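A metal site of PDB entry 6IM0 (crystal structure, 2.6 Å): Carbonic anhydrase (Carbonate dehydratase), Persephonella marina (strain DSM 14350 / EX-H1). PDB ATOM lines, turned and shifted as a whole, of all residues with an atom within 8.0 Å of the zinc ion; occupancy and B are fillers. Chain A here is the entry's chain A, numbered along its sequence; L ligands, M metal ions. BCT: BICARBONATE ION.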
ATOM      1  N   TYR A  25       9.955   6.460  25.726  1.00  0.00           N
ATOM      2  CA  TYR A  25      10.570   7.786  25.485  1.00  0.00           C
ATOM      3  C   TYR A  25      12.094   7.735  25.277  1.00  0.00           C
ATOM      4  O   TYR A  25      12.671   8.729  24.879  1.00  0.00           O
ATOM      5  CB  TYR A  25      10.205   8.774  26.630  1.00  0.00           C
ATOM      6  CG  TYR A  25       8.787   9.295  26.579  1.00  0.00           C
ATOM      7  CD1 TYR A  25       8.398  10.240  25.631  1.00  0.00           C
ATOM      8  CD2 TYR A  25       7.818   8.824  27.460  1.00  0.00           C
ATOM      9  CE1 TYR A  25       7.072  10.696  25.567  1.00  0.00           C
ATOM     10  CE2 TYR A  25       6.489   9.300  27.401  1.00  0.00           C
ATOM     11  CZ  TYR A  25       6.126  10.235  26.466  1.00  0.00           C
ATOM     12  OH  TYR A  25       4.845  10.697  26.409  1.00  0.00           O
ATOM     13  N   THR A  83       3.120   7.966  31.781  1.00  0.00           N
ATOM     14  CA  THR A  83       2.732   9.156  32.522  1.00  0.00           C
ATOM     15  C   THR A  83       2.009   8.788  33.827  1.00  0.00           C
ATOM     16  O   THR A  83       1.883   7.612  34.178  1.00  0.00           O
ATOM     17  CB  THR A  83       1.805  10.031  31.647  1.00  0.00           C
ATOM     18  OG1 THR A  83       1.603  11.329  32.249  1.00  0.00           O
ATOM     19  CG2 THR A  83       0.435   9.348  31.427  1.00  0.00           C
ATOM     20  N   GLN A 105      -9.934  12.659  30.982  1.00  0.00           N
ATOM     21  CA  GLN A 105      -8.767  12.433  31.813  1.00  0.00           C
ATOM     22  C   GLN A 105      -7.774  13.541  31.617  1.00  0.00           C
ATOM     23  O   GLN A 105      -7.782  14.217  30.583  1.00  0.00           O
ATOM     24  CB  GLN A 105      -8.081  11.113  31.420  1.00  0.00           C
ATOM     25  CG  GLN A 105      -7.684  10.977  29.944  1.00  0.00           C
ATOM     26  CD  GLN A 105      -6.209  11.243  29.644  1.00  0.00           C
ATOM     27  OE1 GLN A 105      -5.514  11.967  30.362  1.00  0.00           O
ATOM     28  NE2 GLN A 105      -5.741  10.667  28.554  1.00  0.00           N
ATOM     29  N   PHE A 106      -6.871  13.687  32.572  1.00  0.00           N
ATOM     30  CA  PHE A 106      -5.716  14.555  32.407  1.00  0.00           C
ATOM     31  C   PHE A 106      -4.466  13.896  32.934  1.00  0.00           C
ATOM     32  O   PHE A 106      -4.538  13.039  33.800  1.00  0.00           O
ATOM     33  CB  PHE A 106      -5.939  15.962  33.022  1.00  0.00           C
ATOM     34  CG  PHE A 106      -6.158  15.977  34.520  1.00  0.00           C
ATOM     35  CD1 PHE A 106      -5.067  16.134  35.390  1.00  0.00           C
ATOM     36  CD2 PHE A 106      -7.445  15.933  35.061  1.00  0.00           C
ATOM     37  CE1 PHE A 106      -5.263  16.206  36.762  1.00  0.00           C
ATOM     38  CE2 PHE A 106      -7.651  15.999  36.449  1.00  0.00           C
ATOM     39  CZ  PHE A 106      -6.556  16.143  37.293  1.00  0.00           C
ATOM     40  N   HIS A 107      -3.329  14.282  32.382  1.00  0.00           N
ATOM     41  CA  HIS A 107      -2.048  13.622  32.643  1.00  0.00           C
ATOM     42  C   HIS A 107      -0.897  14.606  32.429  1.00  0.00           C
ATOM     43  O   HIS A 107      -1.130  15.757  32.096  1.00  0.00           O
ATOM     44  CB  HIS A 107      -1.902  12.414  31.725  1.00  0.00           C
ATOM     45  CG  HIS A 107      -1.816  12.798  30.297  1.00  0.00           C
ATOM     46  ND1 HIS A 107      -2.899  12.713  29.433  1.00  0.00           N
ATOM     47  CD2 HIS A 107      -0.783  13.297  29.555  1.00  0.00           C
ATOM     48  CE1 HIS A 107      -2.560  13.128  28.219  1.00  0.00           C
ATOM     49  NE2 HIS A 107      -1.294  13.470  28.310  1.00  0.00           N
ATOM     50  N   PHE A 108       0.337  14.149  32.558  1.00  0.00           N
ATOM     51  CA  PHE A 108       1.484  15.042  32.659  1.00  0.00           C
ATOM     52  C   PHE A 108       2.705  14.589  31.844  1.00  0.00           C
ATOM     53  O   PHE A 108       2.891  13.397  31.557  1.00  0.00           O
ATOM     54  CB  PHE A 108       1.891  15.156  34.152  1.00  0.00           C
ATOM     55  CG  PHE A 108       0.744  15.467  35.039  1.00  0.00           C
ATOM     56  CD1 PHE A 108       0.267  16.768  35.112  1.00  0.00           C
ATOM     57  CD2 PHE A 108       0.094  14.482  35.730  1.00  0.00           C
ATOM     58  CE1 PHE A 108      -0.843  17.082  35.888  1.00  0.00           C
ATOM     59  CE2 PHE A 108      -0.991  14.782  36.541  1.00  0.00           C
ATOM     60  CZ  PHE A 108      -1.481  16.079  36.616  1.00  0.00           C
ATOM     61  N   HIS A 109       3.533  15.560  31.502  1.00  0.00           N
ATOM     62  CA  HIS A 109       4.821  15.323  30.872  1.00  0.00           C
ATOM     63  C   HIS A 109       5.844  16.285  31.490  1.00  0.00           C
ATOM     64  O   HIS A 109       5.489  17.384  31.908  1.00  0.00           O
ATOM     65  CB  HIS A 109       4.791  15.617  29.385  1.00  0.00           C
ATOM     66  CG  HIS A 109       3.710  14.909  28.634  1.00  0.00           C
ATOM     67  ND1 HIS A 109       3.884  13.677  28.037  1.00  0.00           N
ATOM     68  CD2 HIS A 109       2.434  15.277  28.332  1.00  0.00           C
ATOM     69  CE1 HIS A 109       2.787  13.289  27.416  1.00  0.00           C
ATOM     70  NE2 HIS A 109       1.913  14.251  27.606  1.00  0.00           N
ATOM     71  N   GLU A 113       6.138  19.339  26.598  1.00  0.00           N
ATOM     72  CA  GLU A 113       6.139  18.823  25.237  1.00  0.00           C
ATOM     73  C   GLU A 113       6.237  19.948  24.237  1.00  0.00           C
ATOM     74  O   GLU A 113       7.178  20.017  23.441  1.00  0.00           O
ATOM     75  CB  GLU A 113       4.893  17.974  24.976  1.00  0.00           C
ATOM     76  CG  GLU A 113       4.916  16.708  25.830  1.00  0.00           C
ATOM     77  CD  GLU A 113       4.389  15.490  25.117  1.00  0.00           C
ATOM     78  OE1 GLU A 113       3.168  15.414  24.953  1.00  0.00           O
ATOM     79  OE2 GLU A 113       5.208  14.609  24.771  1.00  0.00           O
ATOM     80  N   HIS A 114       5.285  20.880  24.327  1.00  0.00           N
ATOM     81  CA  HIS A 114       5.387  22.148  23.593  1.00  0.00           C
ATOM     82  C   HIS A 114       6.544  23.019  24.080  1.00  0.00           C
ATOM     83  O   HIS A 114       6.864  23.053  25.250  1.00  0.00           O
ATOM     84  CB  HIS A 114       4.085  22.918  23.671  1.00  0.00           C
ATOM     85  CG  HIS A 114       2.960  22.221  22.969  1.00  0.00           C
ATOM     86  ND1 HIS A 114       2.155  21.295  23.605  1.00  0.00           N
ATOM     87  CD2 HIS A 114       2.562  22.245  21.681  1.00  0.00           C
ATOM     88  CE1 HIS A 114       1.281  20.819  22.736  1.00  0.00           C
ATOM     89  NE2 HIS A 114       1.525  21.366  21.558  1.00  0.00           N
ATOM     90  N   GLU A 124       4.347  20.131  31.922  1.00  0.00           N
ATOM     91  CA  GLU A 124       3.196  20.446  31.084  1.00  0.00           C
ATOM     92  C   GLU A 124       2.110  19.427  31.402  1.00  0.00           C
ATOM     93  O   GLU A 124       2.415  18.253  31.624  1.00  0.00           O
ATOM     94  CB  GLU A 124       3.534  20.373  29.605  1.00  0.00           C
ATOM     95  CG  GLU A 124       2.409  20.805  28.652  1.00  0.00           C
ATOM     96  CD  GLU A 124       2.820  20.871  27.170  1.00  0.00           C
ATOM     97  OE1 GLU A 124       3.996  21.175  26.851  1.00  0.00           O
ATOM     98  OE2 GLU A 124       1.940  20.648  26.289  1.00  0.00           O
ATOM     99  N   ALA A 125       0.865  19.895  31.470  1.00  0.00           N
ATOM    100  CA  ALA A 125      -0.300  19.061  31.704  1.00  0.00           C
ATOM    101  C   ALA A 125      -1.217  19.087  30.514  1.00  0.00           C
ATOM    102  O   ALA A 125      -1.382  20.131  29.861  1.00  0.00           O
ATOM    103  CB  ALA A 125      -1.055  19.545  32.922  1.00  0.00           C
ATOM    104  N   HIS A 126      -1.850  17.941  30.270  1.00  0.00           N
ATOM    105  CA  HIS A 126      -2.791  17.783  29.173  1.00  0.00           C
ATOM    106  C   HIS A 126      -4.143  17.337  29.688  1.00  0.00           C
ATOM    107  O   HIS A 126      -4.266  16.336  30.343  1.00  0.00           O
ATOM    108  CB  HIS A 126      -2.265  16.746  28.166  1.00  0.00           C
ATOM    109  CG  HIS A 126      -1.048  17.190  27.437  1.00  0.00           C
ATOM    110  ND1 HIS A 126      -0.153  16.332  26.849  1.00  0.00           N
ATOM    111  CD2 HIS A 126      -0.554  18.440  27.253  1.00  0.00           C
ATOM    112  CE1 HIS A 126       0.818  17.036  26.291  1.00  0.00           C
ATOM    113  NE2 HIS A 126       0.607  18.316  26.543  1.00  0.00           N
ATOM    114  N   PHE A 127      -5.169  18.088  29.365  1.00  0.00           N
ATOM    115  CA  PHE A 127      -6.522  17.746  29.717  1.00  0.00           C
ATOM    116  C   PHE A 127      -7.206  17.245  28.451  1.00  0.00           C
ATOM    117  O   PHE A 127      -7.474  18.002  27.539  1.00  0.00           O
ATOM    118  CB  PHE A 127      -7.230  18.976  30.325  1.00  0.00           C
ATOM    119  CG  PHE A 127      -6.540  19.495  31.565  1.00  0.00           C
ATOM    120  CD1 PHE A 127      -5.413  20.286  31.478  1.00  0.00           C
ATOM    121  CD2 PHE A 127      -6.998  19.130  32.831  1.00  0.00           C
ATOM    122  CE1 PHE A 127      -4.736  20.720  32.628  1.00  0.00           C
ATOM    123  CE2 PHE A 127      -6.347  19.549  33.984  1.00  0.00           C
ATOM    124  CZ  PHE A 127      -5.197  20.358  33.881  1.00  0.00           C
ATOM    125  N   VAL A 128      -7.486  15.940  28.418  1.00  0.00           N
ATOM    126  CA  VAL A 128      -7.946  15.275  27.213  1.00  0.00           C
ATOM    127  C   VAL A 128      -9.449  15.184  27.209  1.00  0.00           C
ATOM    128  O   VAL A 128     -10.027  14.602  28.131  1.00  0.00           O
ATOM    129  CB  VAL A 128      -7.369  13.871  27.080  1.00  0.00           C
ATOM    130  CG1 VAL A 128      -7.842  13.240  25.767  1.00  0.00           C
ATOM    131  CG2 VAL A 128      -5.846  13.911  27.092  1.00  0.00           C
ATOM    132  N   VAL A 138      -7.571  18.780  23.287  1.00  0.00           N
ATOM    133  CA  VAL A 138      -6.680  18.715  24.408  1.00  0.00           C
ATOM    134  C   VAL A 138      -6.366  20.150  24.861  1.00  0.00           C
ATOM    135  O   VAL A 138      -5.962  20.987  24.054  1.00  0.00           O
ATOM    136  CB  VAL A 138      -5.400  17.963  24.035  1.00  0.00           C
ATOM    137  CG1 VAL A 138      -4.488  17.799  25.234  1.00  0.00           C
ATOM    138  CG2 VAL A 138      -5.739  16.598  23.492  1.00  0.00           C
ATOM    139  N   ILE A 139      -6.511  20.428  26.153  1.00  0.00           N
ATOM    140  CA  ILE A 139      -6.048  21.675  26.709  1.00  0.00           C
ATOM    141  C   ILE A 139      -4.683  21.409  27.293  1.00  0.00           C
ATOM    142  O   ILE A 139      -4.496  20.465  28.058  1.00  0.00           O
ATOM    143  CB  ILE A 139      -6.974  22.249  27.785  1.00  0.00           C
ATOM    144  CG1 ILE A 139      -8.290  22.692  27.161  1.00  0.00           C
ATOM    145  CG2 ILE A 139      -6.307  23.454  28.485  1.00  0.00           C
ATOM    146  CD1 ILE A 139      -9.327  23.210  28.132  1.00  0.00           C
ATOM    147  N   SER A 191      -1.972  16.606  16.754  1.00  0.00           N
ATOM    148  CA  SER A 191      -2.111  15.178  17.019  1.00  0.00           C
ATOM    149  C   SER A 191      -1.960  14.809  18.469  1.00  0.00           C
ATOM    150  O   SER A 191      -1.514  15.603  19.275  1.00  0.00           O
ATOM    151  CB  SER A 191      -1.043  14.391  16.220  1.00  0.00           C
ATOM    152  OG  SER A 191       0.249  14.427  16.840  1.00  0.00           O
ATOM    153  N   LEU A 192      -2.281  13.554  18.790  1.00  0.00           N
ATOM    154  CA  LEU A 192      -1.816  12.987  20.037  1.00  0.00           C
ATOM    155  C   LEU A 192      -0.287  12.942  20.059  1.00  0.00           C
ATOM    156  O   LEU A 192       0.330  12.752  19.032  1.00  0.00           O
ATOM    157  CB  LEU A 192      -2.388  11.596  20.232  1.00  0.00           C
ATOM    158  CG  LEU A 192      -3.908  11.500  20.489  1.00  0.00           C
ATOM    159  CD1 LEU A 192      -4.296  10.021  20.660  1.00  0.00           C
ATOM    160  CD2 LEU A 192      -4.348  12.298  21.715  1.00  0.00           C
ATOM    161  N   THR A 193       0.297  13.147  21.227  1.00  0.00           N
ATOM    162  CA  THR A 193       1.756  13.121  21.373  1.00  0.00           C
ATOM    163  C   THR A 193       2.341  11.746  21.756  1.00  0.00           C
ATOM    164  O   THR A 193       3.560  11.616  21.905  1.00  0.00           O
ATOM    165  CB  THR A 193       2.258  14.137  22.420  1.00  0.00           C
ATOM    166  OG1 THR A 193       1.829  13.760  23.751  1.00  0.00           O
ATOM    167  CG2 THR A 193       1.763  15.506  22.082  1.00  0.00           C
ATOM    168  N   THR A 194       1.468  10.770  21.966  1.00  0.00           N
ATOM    169  CA  THR A 194       1.871   9.399  22.206  1.00  0.00           C
ATOM    170  C   THR A 194       1.231   8.523  21.132  1.00  0.00           C
ATOM    171  O   THR A 194       0.125   8.864  20.682  1.00  0.00           O
ATOM    172  CB  THR A 194       1.397   8.891  23.572  1.00  0.00           C
ATOM    173  OG1 THR A 194      -0.035   8.868  23.639  1.00  0.00           O
ATOM    174  CG2 THR A 194       1.935   9.753  24.674  1.00  0.00           C
ATOM    175  N   TRP A 203      -5.821  21.391  19.536  1.00  0.00           N
ATOM    176  CA  TRP A 203      -4.956  21.766  20.637  1.00  0.00           C
ATOM    177  C   TRP A 203      -5.287  23.171  21.143  1.00  0.00           C
ATOM    178  O   TRP A 203      -5.284  24.126  20.381  1.00  0.00           O
ATOM    179  CB  TRP A 203      -3.489  21.688  20.207  1.00  0.00           C
ATOM    180  CG  TRP A 203      -2.916  20.331  20.426  1.00  0.00           C
ATOM    181  CD1 TRP A 203      -2.746  19.362  19.485  1.00  0.00           C
ATOM    182  CD2 TRP A 203      -2.483  19.770  21.667  1.00  0.00           C
ATOM    183  NE1 TRP A 203      -2.213  18.246  20.053  1.00  0.00           N
ATOM    184  CE2 TRP A 203      -2.055  18.459  21.395  1.00  0.00           C
ATOM    185  CE3 TRP A 203      -2.413  20.259  22.976  1.00  0.00           C
ATOM    186  CZ2 TRP A 203      -1.557  17.619  22.377  1.00  0.00           C
ATOM    187  CZ3 TRP A 203      -1.909  19.428  23.966  1.00  0.00           C
ATOM    188  CH2 TRP A 203      -1.482  18.126  23.659  1.00  0.00           C
ATOM    189  N   THR A 228       9.753  12.641  29.825  1.00  0.00           N
ATOM    190  CA  THR A 228       8.471  12.102  29.341  1.00  0.00           C
ATOM    191  C   THR A 228       7.872  12.958  28.186  1.00  0.00           C
ATOM    192  O   THR A 228       6.633  13.028  28.013  1.00  0.00           O
ATOM    193  CB  THR A 228       7.456  11.980  30.506  1.00  0.00           C
ATOM    194  OG1 THR A 228       7.682  13.034  31.461  1.00  0.00           O
ATOM    195  CG2 THR A 228       7.627  10.636  31.191  1.00  0.00           C
HETATM  196  C   BCT L   1      -1.436  13.912  24.531  1.00  0.00           C
HETATM  197  O1  BCT L   1      -2.176  14.497  25.359  1.00  0.00           O
HETATM  198  O2  BCT L   1      -1.594  13.923  23.295  1.00  0.00           O
HETATM  199  O3  BCT L   1      -0.299  13.233  25.103  1.00  0.00           O
HETATM  200 ZN    ZN M   1      -0.059  14.296  26.820  1.00  0.00          ZN
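Glu 113 touches the zinc ion (OE1 to ZN, 3.9 Å). Thr 193 touches the zinc ion. Of the 22 residues printed, 5 come within 4 Å of the zinc ion. The nearest printed residue that does not touch the zinc ion is Trp 203 (5.2 Å).
The zinc ion is bound by an oxygen (O3) of the ligand (2.0 Å), a ring nitrogen (ND1) of His 126 (2.0 Å), a ring nitrogen (NE2) of His 107 (2.1 Å), a ring nitrogen (NE2) of His 109 (2.1 Å) and an oxygen (O1) of the ligand (2.6 Å).
The backbone carbonyl oxygen (O) of Glu 124 is in hydrogen-bond range of the backbone NH (N) of His 109, 2.9 Å away. The backbone NH of Glu 113 lies within hydrogen-bond range of the side-chain carboxylate of Glu 124 (2.8 Å). ND1 of His 107 sits at hydrogen-bond distance from OE1 of Gln 105. OE1 of Glu 113 is in hydrogen-bond range of OG1 of Thr 193 (2.4 Å). The side-chain carboxylate (OE1) of Glu 113 sits close to a ring nitrogen (NE2) of His 109 (3.2 Å). A ring nitrogen (ND1) of His 109 is in hydrogen-bond range of the backbone carbonyl oxygen (O) of Thr 228 (2.8 Å). A ring nitrogen (NE2) of His 126 is in hydrogen-bond range of the side-chain carboxylate (OE2) of Glu 124, 2.7 Å away.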
